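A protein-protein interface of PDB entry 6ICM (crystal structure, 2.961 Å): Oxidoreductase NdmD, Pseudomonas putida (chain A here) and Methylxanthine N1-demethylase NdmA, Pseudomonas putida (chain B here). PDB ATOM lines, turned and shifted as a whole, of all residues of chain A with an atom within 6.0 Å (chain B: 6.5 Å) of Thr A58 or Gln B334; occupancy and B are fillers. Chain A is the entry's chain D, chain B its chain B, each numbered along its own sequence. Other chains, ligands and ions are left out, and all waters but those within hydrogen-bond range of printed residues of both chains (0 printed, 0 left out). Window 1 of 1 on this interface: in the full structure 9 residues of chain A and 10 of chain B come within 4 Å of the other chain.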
ATOM      1  N   GLY A  39      24.750 -27.221   9.859  1.00  0.00           N
ATOM      2  CA  GLY A  39      23.990 -27.000  11.078  1.00  0.00           C
ATOM      3  C   GLY A  39      22.629 -26.345  10.978  1.00  0.00           C
ATOM      4  O   GLY A  39      22.393 -25.361  11.685  1.00  0.00           O
ATOM      5  N   VAL A  40      21.704 -26.876  10.171  1.00  0.00           N
ATOM      6  CA  VAL A  40      20.500 -26.100   9.878  1.00  0.00           C
ATOM      7  C   VAL A  40      19.182 -26.820  10.140  1.00  0.00           C
ATOM      8  O   VAL A  40      18.221 -26.191  10.598  1.00  0.00           O
ATOM      9  CB  VAL A  40      20.530 -25.560   8.431  1.00  0.00           C
ATOM     10  CG1 VAL A  40      20.046 -26.588   7.405  1.00  0.00           C
ATOM     11  CG2 VAL A  40      19.714 -24.270   8.340  1.00  0.00           C
ATOM     12  N   HIS A  56      28.365 -23.803  15.973  1.00  0.00           N
ATOM     13  CA  HIS A  56      28.578 -23.459  14.574  1.00  0.00           C
ATOM     14  C   HIS A  56      27.321 -23.711  13.772  1.00  0.00           C
ATOM     15  O   HIS A  56      27.402 -23.803  12.554  1.00  0.00           O
ATOM     16  CB  HIS A  56      29.711 -24.271  13.960  1.00  0.00           C
ATOM     17  CG  HIS A  56      31.013 -24.118  14.674  1.00  0.00           C
ATOM     18  ND1 HIS A  56      31.833 -25.192  14.934  1.00  0.00           N
ATOM     19  CD2 HIS A  56      31.644 -23.032  15.182  1.00  0.00           C
ATOM     20  CE1 HIS A  56      32.905 -24.782  15.583  1.00  0.00           C
ATOM     21  NE2 HIS A  56      32.817 -23.475  15.745  1.00  0.00           N
ATOM     22  N   ASP A  57      26.170 -23.830  14.425  1.00  0.00           N
ATOM     23  CA  ASP A  57      24.943 -24.140  13.720  1.00  0.00           C
ATOM     24  C   ASP A  57      24.219 -22.857  13.342  1.00  0.00           C
ATOM     25  O   ASP A  57      24.592 -21.749  13.741  1.00  0.00           O
ATOM     26  CB  ASP A  57      24.039 -25.003  14.588  1.00  0.00           C
ATOM     27  CG  ASP A  57      23.617 -24.286  15.844  1.00  0.00           C
ATOM     28  OD1 ASP A  57      24.479 -24.152  16.743  1.00  0.00           O
ATOM     29  OD2 ASP A  57      22.446 -23.836  15.927  1.00  0.00           O
ATOM     30  N   THR A  58      23.157 -23.032  12.567  1.00  0.00           N
ATOM     31  CA  THR A  58      22.225 -21.981  12.216  1.00  0.00           C
ATOM     32  C   THR A  58      20.807 -22.425  12.541  1.00  0.00           C
ATOM     33  O   THR A  58      19.849 -22.128  11.818  1.00  0.00           O
ATOM     34  CB  THR A  58      22.380 -21.583  10.745  1.00  0.00           C
ATOM     35  OG1 THR A  58      22.254 -22.733   9.891  1.00  0.00           O
ATOM     36  CG2 THR A  58      23.747 -20.903  10.506  1.00  0.00           C
ATOM     37  N   TYR A  59      20.664 -23.155  13.638  1.00  0.00           N
ATOM     38  CA  TYR A  59      19.366 -23.583  14.138  1.00  0.00           C
ATOM     39  C   TYR A  59      19.058 -23.039  15.522  1.00  0.00           C
ATOM     40  O   TYR A  59      17.915 -22.671  15.800  1.00  0.00           O
ATOM     41  CB  TYR A  59      19.293 -25.114  14.167  1.00  0.00           C
ATOM     42  CG  TYR A  59      18.002 -25.648  14.741  1.00  0.00           C
ATOM     43  CD1 TYR A  59      16.838 -25.687  13.984  1.00  0.00           C
ATOM     44  CD2 TYR A  59      17.946 -26.115  16.042  1.00  0.00           C
ATOM     45  CE1 TYR A  59      15.642 -26.171  14.519  1.00  0.00           C
ATOM     46  CE2 TYR A  59      16.769 -26.592  16.579  1.00  0.00           C
ATOM     47  CZ  TYR A  59      15.615 -26.618  15.821  1.00  0.00           C
ATOM     48  OH  TYR A  59      14.449 -27.116  16.386  1.00  0.00           O
ATOM     49  N   LEU A  60      20.041 -22.970  16.409  1.00  0.00           N
ATOM     50  CA  LEU A  60      19.754 -22.569  17.776  1.00  0.00           C
ATOM     51  C   LEU A  60      19.756 -21.062  17.917  1.00  0.00           C
ATOM     52  O   LEU A  60      20.661 -20.382  17.425  1.00  0.00           O
ATOM     53  CB  LEU A  60      20.762 -23.184  18.747  1.00  0.00           C
ATOM     54  CG  LEU A  60      20.545 -24.682  18.946  1.00  0.00           C
ATOM     55  CD1 LEU A  60      21.796 -25.323  19.428  1.00  0.00           C
ATOM     56  CD2 LEU A  60      19.397 -24.962  19.921  1.00  0.00           C
ATOM     57  N   ARG A  65      21.801 -20.971  22.477  1.00  0.00           N
ATOM     58  CA  ARG A  65      23.244 -21.212  22.446  1.00  0.00           C
ATOM     59  C   ARG A  65      23.892 -20.824  23.765  1.00  0.00           C
ATOM     60  O   ARG A  65      24.783 -21.528  24.261  1.00  0.00           O
ATOM     61  CB  ARG A  65      23.923 -20.460  21.289  1.00  0.00           C
ATOM     62  CG  ARG A  65      23.038 -20.132  20.104  1.00  0.00           C
ATOM     63  CD  ARG A  65      23.693 -20.356  18.728  1.00  0.00           C
ATOM     64  NE  ARG A  65      24.987 -19.698  18.542  1.00  0.00           N
ATOM     65  CZ  ARG A  65      25.747 -19.842  17.451  1.00  0.00           C
ATOM     66  NH1 ARG A  65      25.344 -20.629  16.455  1.00  0.00           N
ATOM     67  NH2 ARG A  65      26.914 -19.210  17.351  1.00  0.00           N
ATOM     68  N   VAL A  75      28.043 -30.144  13.738  1.00  0.00           N
ATOM     69  CA  VAL A  75      28.916 -29.039  13.352  1.00  0.00           C
ATOM     70  C   VAL A  75      29.528 -28.360  14.566  1.00  0.00           C
ATOM     71  O   VAL A  75      30.513 -27.628  14.436  1.00  0.00           O
ATOM     72  CB  VAL A  75      28.175 -28.002  12.479  1.00  0.00           C
ATOM     73  CG1 VAL A  75      27.582 -28.640  11.228  1.00  0.00           C
ATOM     74  CG2 VAL A  75      27.103 -27.253  13.270  1.00  0.00           C
ATOM     75  N   ILE B 210      22.104 -16.813   3.185  1.00  0.00           N
ATOM     76  CA  ILE B 210      21.566 -17.145   4.483  1.00  0.00           C
ATOM     77  C   ILE B 210      21.386 -15.821   5.179  1.00  0.00           C
ATOM     78  O   ILE B 210      22.259 -14.955   5.089  1.00  0.00           O
ATOM     79  CB  ILE B 210      22.521 -18.076   5.247  1.00  0.00           C
ATOM     80  CG1 ILE B 210      23.117 -19.128   4.301  1.00  0.00           C
ATOM     81  CG2 ILE B 210      21.809 -18.703   6.414  1.00  0.00           C
ATOM     82  CD1 ILE B 210      22.108 -20.013   3.539  1.00  0.00           C
ATOM     83  N   MET B 213      17.259 -14.045  11.009  1.00  0.00           N
ATOM     84  CA  MET B 213      15.819 -13.935  11.163  1.00  0.00           C
ATOM     85  C   MET B 213      15.499 -13.576  12.601  1.00  0.00           C
ATOM     86  O   MET B 213      16.045 -14.181  13.530  1.00  0.00           O
ATOM     87  CB  MET B 213      15.133 -15.242  10.795  1.00  0.00           C
ATOM     88  CG  MET B 213      15.603 -15.774   9.477  1.00  0.00           C
ATOM     89  SD  MET B 213      14.898 -17.381   9.108  1.00  0.00           S
ATOM     90  CE  MET B 213      13.127 -17.136   9.041  1.00  0.00           C
ATOM     91  N   ARG B 215      12.412 -12.920  15.554  1.00  0.00           N
ATOM     92  CA  ARG B 215      11.030 -12.978  16.004  1.00  0.00           C
ATOM     93  C   ARG B 215      10.763 -11.667  16.715  1.00  0.00           C
ATOM     94  O   ARG B 215      11.482 -11.319  17.656  1.00  0.00           O
ATOM     95  CB  ARG B 215      10.772 -14.136  16.971  1.00  0.00           C
ATOM     96  CG  ARG B 215      10.994 -15.521  16.447  1.00  0.00           C
ATOM     97  CD  ARG B 215      10.696 -16.586  17.498  1.00  0.00           C
ATOM     98  NE  ARG B 215      11.329 -17.834  17.089  1.00  0.00           N
ATOM     99  CZ  ARG B 215      11.045 -19.042  17.569  1.00  0.00           C
ATOM    100  NH1 ARG B 215      10.113 -19.203  18.504  1.00  0.00           N
ATOM    101  NH2 ARG B 215      11.693 -20.098  17.081  1.00  0.00           N
ATOM    102  N   PHE B 220       7.896 -12.820  11.836  1.00  0.00           N
ATOM    103  CA  PHE B 220       9.243 -13.130  11.400  1.00  0.00           C
ATOM    104  C   PHE B 220       9.723 -11.981  10.536  1.00  0.00           C
ATOM    105  O   PHE B 220       8.947 -11.447   9.735  1.00  0.00           O
ATOM    106  CB  PHE B 220       9.295 -14.412  10.576  1.00  0.00           C
ATOM    107  CG  PHE B 220       9.994 -15.551  11.248  1.00  0.00           C
ATOM    108  CD1 PHE B 220      11.371 -15.657  11.218  1.00  0.00           C
ATOM    109  CD2 PHE B 220       9.278 -16.595  11.778  1.00  0.00           C
ATOM    110  CE1 PHE B 220      12.014 -16.728  11.807  1.00  0.00           C
ATOM    111  CE2 PHE B 220       9.929 -17.675  12.337  1.00  0.00           C
ATOM    112  CZ  PHE B 220      11.287 -17.737  12.354  1.00  0.00           C
ATOM    113  N   MET B 247       2.906 -14.455  12.007  1.00  0.00           N
ATOM    114  CA  MET B 247       2.671 -15.906  12.111  1.00  0.00           C
ATOM    115  C   MET B 247       1.194 -16.214  12.303  1.00  0.00           C
ATOM    116  O   MET B 247       0.522 -15.509  13.037  1.00  0.00           O
ATOM    117  CB  MET B 247       3.470 -16.508  13.266  1.00  0.00           C
ATOM    118  CG  MET B 247       4.954 -16.450  13.083  1.00  0.00           C
ATOM    119  SD  MET B 247       5.548 -17.592  11.830  1.00  0.00           S
ATOM    120  CE  MET B 247       5.038 -19.175  12.498  1.00  0.00           C
ATOM    121  N   VAL B 327      21.566 -26.088   3.769  1.00  0.00           N
ATOM    122  CA  VAL B 327      21.710 -24.817   4.471  1.00  0.00           C
ATOM    123  C   VAL B 327      20.879 -23.704   3.830  1.00  0.00           C
ATOM    124  O   VAL B 327      20.551 -22.708   4.490  1.00  0.00           O
ATOM    125  CB  VAL B 327      23.203 -24.453   4.550  1.00  0.00           C
ATOM    126  CG1 VAL B 327      23.928 -25.493   5.366  1.00  0.00           C
ATOM    127  CG2 VAL B 327      23.795 -24.373   3.170  1.00  0.00           C
ATOM    128  N   ASP B 329      17.876 -23.877   3.351  1.00  0.00           N
ATOM    129  CA  ASP B 329      16.523 -24.006   3.860  1.00  0.00           C
ATOM    130  C   ASP B 329      16.337 -23.369   5.237  1.00  0.00           C
ATOM    131  O   ASP B 329      15.356 -23.683   5.924  1.00  0.00           O
ATOM    132  CB  ASP B 329      16.112 -25.479   3.891  1.00  0.00           C
ATOM    133  CG  ASP B 329      16.197 -26.149   2.514  1.00  0.00           C
ATOM    134  OD1 ASP B 329      15.954 -25.480   1.471  1.00  0.00           O
ATOM    135  OD2 ASP B 329      16.513 -27.365   2.476  1.00  0.00           O
ATOM    136  N   LYS B 330      17.224 -22.451   5.636  1.00  0.00           N
ATOM    137  CA  LYS B 330      17.114 -21.850   6.963  1.00  0.00           C
ATOM    138  C   LYS B 330      15.699 -21.361   7.249  1.00  0.00           C
ATOM    139  O   LYS B 330      15.116 -21.711   8.286  1.00  0.00           O
ATOM    140  CB  LYS B 330      18.103 -20.698   7.138  1.00  0.00           C
ATOM    141  CG  LYS B 330      17.981 -20.084   8.522  1.00  0.00           C
ATOM    142  CD  LYS B 330      19.129 -19.165   8.867  1.00  0.00           C
ATOM    143  CE  LYS B 330      18.896 -18.498  10.221  1.00  0.00           C
ATOM    144  NZ  LYS B 330      19.876 -17.410  10.478  1.00  0.00           N
ATOM    145  N   VAL B 331      15.128 -20.554   6.336  1.00  0.00           N
ATOM    146  CA  VAL B 331      13.807 -19.961   6.574  1.00  0.00           C
ATOM    147  C   VAL B 331      12.758 -21.051   6.806  1.00  0.00           C
ATOM    148  O   VAL B 331      11.923 -20.951   7.721  1.00  0.00           O
ATOM    149  CB  VAL B 331      13.409 -19.029   5.405  1.00  0.00           C
ATOM    150  CG1 VAL B 331      12.063 -18.377   5.651  1.00  0.00           C
ATOM    151  CG2 VAL B 331      14.446 -17.952   5.159  1.00  0.00           C
ATOM    152  N   SER B 332      12.779 -22.116   5.989  1.00  0.00           N
ATOM    153  CA  SER B 332      11.747 -23.141   6.149  1.00  0.00           C
ATOM    154  C   SER B 332      11.894 -23.860   7.484  1.00  0.00           C
ATOM    155  O   SER B 332      10.896 -24.090   8.174  1.00  0.00           O
ATOM    156  CB  SER B 332      11.747 -24.136   4.981  1.00  0.00           C
ATOM    157  OG  SER B 332      13.004 -24.744   4.795  1.00  0.00           O
ATOM    158  N   ILE B 333      13.129 -24.166   7.895  1.00  0.00           N
ATOM    159  CA  ILE B 333      13.345 -24.810   9.189  1.00  0.00           C
ATOM    160  C   ILE B 333      12.913 -23.896  10.338  1.00  0.00           C
ATOM    161  O   ILE B 333      12.123 -24.293  11.209  1.00  0.00           O
ATOM    162  CB  ILE B 333      14.815 -25.222   9.333  1.00  0.00           C
ATOM    163  CG1 ILE B 333      15.162 -26.340   8.338  1.00  0.00           C
ATOM    164  CG2 ILE B 333      15.106 -25.611  10.763  1.00  0.00           C
ATOM    165  CD1 ILE B 333      14.271 -27.550   8.433  1.00  0.00           C
ATOM    166  N   GLN B 334      13.428 -22.660  10.370  1.00  0.00           N
ATOM    167  CA  GLN B 334      13.042 -21.721  11.424  1.00  0.00           C
ATOM    168  C   GLN B 334      11.527 -21.562  11.510  1.00  0.00           C
ATOM    169  O   GLN B 334      10.964 -21.437  12.609  1.00  0.00           O
ATOM    170  CB  GLN B 334      13.716 -20.365  11.193  1.00  0.00           C
ATOM    171  CG  GLN B 334      15.157 -20.339  11.650  1.00  0.00           C
ATOM    172  CD  GLN B 334      15.323 -21.003  13.009  1.00  0.00           C
ATOM    173  OE1 GLN B 334      14.617 -20.668  13.983  1.00  0.00           O
ATOM    174  NE2 GLN B 334      16.235 -21.976  13.079  1.00  0.00           N
ATOM    175  N   TYR B 335      10.854 -21.563  10.356  1.00  0.00           N
ATOM    176  CA  TYR B 335       9.396 -21.478  10.328  1.00  0.00           C
ATOM    177  C   TYR B 335       8.772 -22.680  11.036  1.00  0.00           C
ATOM    178  O   TYR B 335       7.847 -22.534  11.846  1.00  0.00           O
ATOM    179  CB  TYR B 335       8.924 -21.376   8.867  1.00  0.00           C
ATOM    180  CG  TYR B 335       7.420 -21.357   8.671  1.00  0.00           C
ATOM    181  CD1 TYR B 335       6.638 -20.346   9.202  1.00  0.00           C
ATOM    182  CD2 TYR B 335       6.783 -22.349   7.936  1.00  0.00           C
ATOM    183  CE1 TYR B 335       5.248 -20.334   9.022  1.00  0.00           C
ATOM    184  CE2 TYR B 335       5.389 -22.340   7.748  1.00  0.00           C
ATOM    185  CZ  TYR B 335       4.638 -21.335   8.295  1.00  0.00           C
ATOM    186  OH  TYR B 335       3.280 -21.332   8.107  1.00  0.00           O
ATOM    187  N   ARG B 336       9.282 -23.879  10.745  1.00  0.00           N
ATOM    188  CA  ARG B 336       8.726 -25.091  11.330  1.00  0.00           C
ATOM    189  C   ARG B 336       9.051 -25.179  12.807  1.00  0.00           C
ATOM    190  O   ARG B 336       8.217 -25.642  13.604  1.00  0.00           O
ATOM    191  CB  ARG B 336       9.253 -26.305  10.579  1.00  0.00           C
ATOM    192  CG  ARG B 336       9.046 -26.223   9.087  1.00  0.00           C
ATOM    193  CD  ARG B 336       9.422 -27.519   8.423  1.00  0.00           C
ATOM    194  NE  ARG B 336       8.892 -27.623   7.080  1.00  0.00           N
ATOM    195  CZ  ARG B 336       9.271 -28.590   6.261  1.00  0.00           C
ATOM    196  NH1 ARG B 336      10.172 -29.475   6.696  1.00  0.00           N
ATOM    197  NH2 ARG B 336       8.770 -28.706   5.028  1.00  0.00           N
ATOM    198  N   LYS B 337      10.251 -24.721  13.186  1.00  0.00           N
ATOM    199  CA  LYS B 337      10.614 -24.697  14.596  1.00  0.00           C
ATOM    200  C   LYS B 337       9.581 -23.914  15.399  1.00  0.00           C
ATOM    201  O   LYS B 337       9.064 -24.402  16.418  1.00  0.00           O
ATOM    202  CB  LYS B 337      12.015 -24.108  14.763  1.00  0.00           C
ATOM    203  CG  LYS B 337      12.495 -24.045  16.210  1.00  0.00           C
ATOM    204  CD  LYS B 337      13.946 -23.588  16.279  1.00  0.00           C
ATOM    205  CE  LYS B 337      14.332 -23.154  17.688  1.00  0.00           C
ATOM    206  NZ  LYS B 337      15.727 -22.619  17.735  1.00  0.00           N
ATOM    207  N   TRP B 338       9.206 -22.723  14.896  1.00  0.00           N
ATOM    208  CA  TRP B 338       8.319 -21.842  15.644  1.00  0.00           C
ATOM    209  C   TRP B 338       6.896 -22.379  15.661  1.00  0.00           C
ATOM    210  O   TRP B 338       6.205 -22.288  16.686  1.00  0.00           O
ATOM    211  CB  TRP B 338       8.375 -20.430  15.068  1.00  0.00           C
ATOM    212  CG  TRP B 338       7.782 -19.350  15.973  1.00  0.00           C
ATOM    213  CD1 TRP B 338       7.171 -19.540  17.181  1.00  0.00           C
ATOM    214  CD2 TRP B 338       7.754 -17.923  15.731  1.00  0.00           C
ATOM    215  NE1 TRP B 338       6.764 -18.334  17.700  1.00  0.00           N
ATOM    216  CE2 TRP B 338       7.110 -17.327  16.833  1.00  0.00           C
ATOM    217  CE3 TRP B 338       8.213 -17.095  14.687  1.00  0.00           C
ATOM    218  CZ2 TRP B 338       6.898 -15.946  16.915  1.00  0.00           C
ATOM    219  CZ3 TRP B 338       8.006 -15.725  14.779  1.00  0.00           C
ATOM    220  CH2 TRP B 338       7.355 -15.170  15.879  1.00  0.00           C
ATOM    221  N   LEU B 339       6.436 -22.956  14.553  1.00  0.00           N
ATOM    222  CA  LEU B 339       5.095 -23.517  14.589  1.00  0.00           C
ATOM    223  C   LEU B 339       5.010 -24.653  15.592  1.00  0.00           C
ATOM    224  O   LEU B 339       4.025 -24.750  16.327  1.00  0.00           O
ATOM    225  CB  LEU B 339       4.632 -23.998  13.219  1.00  0.00           C
ATOM    226  CG  LEU B 339       4.403 -22.932  12.141  1.00  0.00           C
ATOM    227  CD1 LEU B 339       4.288 -23.569  10.807  1.00  0.00           C
ATOM    228  CD2 LEU B 339       3.141 -22.206  12.443  1.00  0.00           C
ATOM    229  N   GLU B 363      18.151 -12.085  16.091  1.00  0.00           N
ATOM    230  CA  GLU B 363      19.381 -12.665  15.590  1.00  0.00           C
ATOM    231  C   GLU B 363      20.255 -11.652  14.872  1.00  0.00           C
ATOM    232  O   GLU B 363      21.466 -11.865  14.779  1.00  0.00           O
ATOM    233  CB  GLU B 363      19.070 -13.819  14.624  1.00  0.00           C
ATOM    234  CG  GLU B 363      20.242 -14.752  14.345  1.00  0.00           C
ATOM    235  CD  GLU B 363      19.982 -15.684  13.178  1.00  0.00           C
ATOM    236  OE1 GLU B 363      20.757 -15.633  12.190  1.00  0.00           O
ATOM    237  OE2 GLU B 363      18.994 -16.454  13.253  1.00  0.00           O
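O of Tyr A59 is in hydrogen-bond range of NE2 of Gln B334 (3.3 Å). The side-chain amino group (NZ) of Lys B337 is in hydrogen-bond range of the backbone carbonyl oxygen (O) of Tyr A59 (2.9 Å).
NZ of Lys B330 lies within salt-bridge range of OE1 of Glu B363 (2.6 Å). The backbone carbonyl oxygen of Gly A39 is in hydrogen-bond range of the backbone NH of Thr A58 (2.6 Å). N of Tyr A59 sits at hydrogen-bond distance from O of Gly A39. The backbone NH (N) of Tyr A59 is in hydrogen-bond range of the side-chain carboxylate (OD2) of Asp A57 (3.0 Å).
CG1 of Val A40 touches CA of Val B327, 3.8 Å away. Val A40 touches Lys B330 (CG2 to CA, 3.8 Å). CG2 of Ile B333 touches O of Val A40, at 3.2 Å. Gln B334 touches Thr A58. CD1 of Tyr A59 touches CG2 of Ile B333, 3.7 Å away.
Thr A58 touches one residue of chain B. Of the printed residues of chain A, Gln B334 touches Thr A58 (3.8 Å) and Tyr A59 (3.3 Å). Printed residues of chain A within 4 Å of Val B327: Val A40 (3.8 Å). Of the printed residues of chain B, Tyr A59 touches Ile B333, Gln B334 and Lys B337. Of the printed residues of chain A, Lys B330 touches Val A40. Printed residues of chain A within 4 Å of Lys B337: Tyr A59 (2.9 Å). Of the printed residues of chain B, Val A40 touches Val B327, Lys B330 and Ile B333. Met B247 touches none of the printed residues of chain A. Glu B363 touches none of the printed residues of chain A. The nearest residue of chain B that does not touch Thr A58 is Lys B330 (4.1 Å). The nearest printed residue of chain B that does not touch Val A40 is Asp B329 (4.7 Å).
Hydrophobic or aromatic side chains of chain A within 4 Å of the printed part of chain B: Val A40 and Tyr A59. Of the 18 printed residues of chain B, 5 touch a printed residue of chain A. Printed residues of chain B that touch a printed residue of chain A: Val B327, Lys B330, Ile B333, Gln B334 and Lys B337. Hydrophobic or aromatic side chains of chain B within 4 Å of the printed part of chain A: Ile B333.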
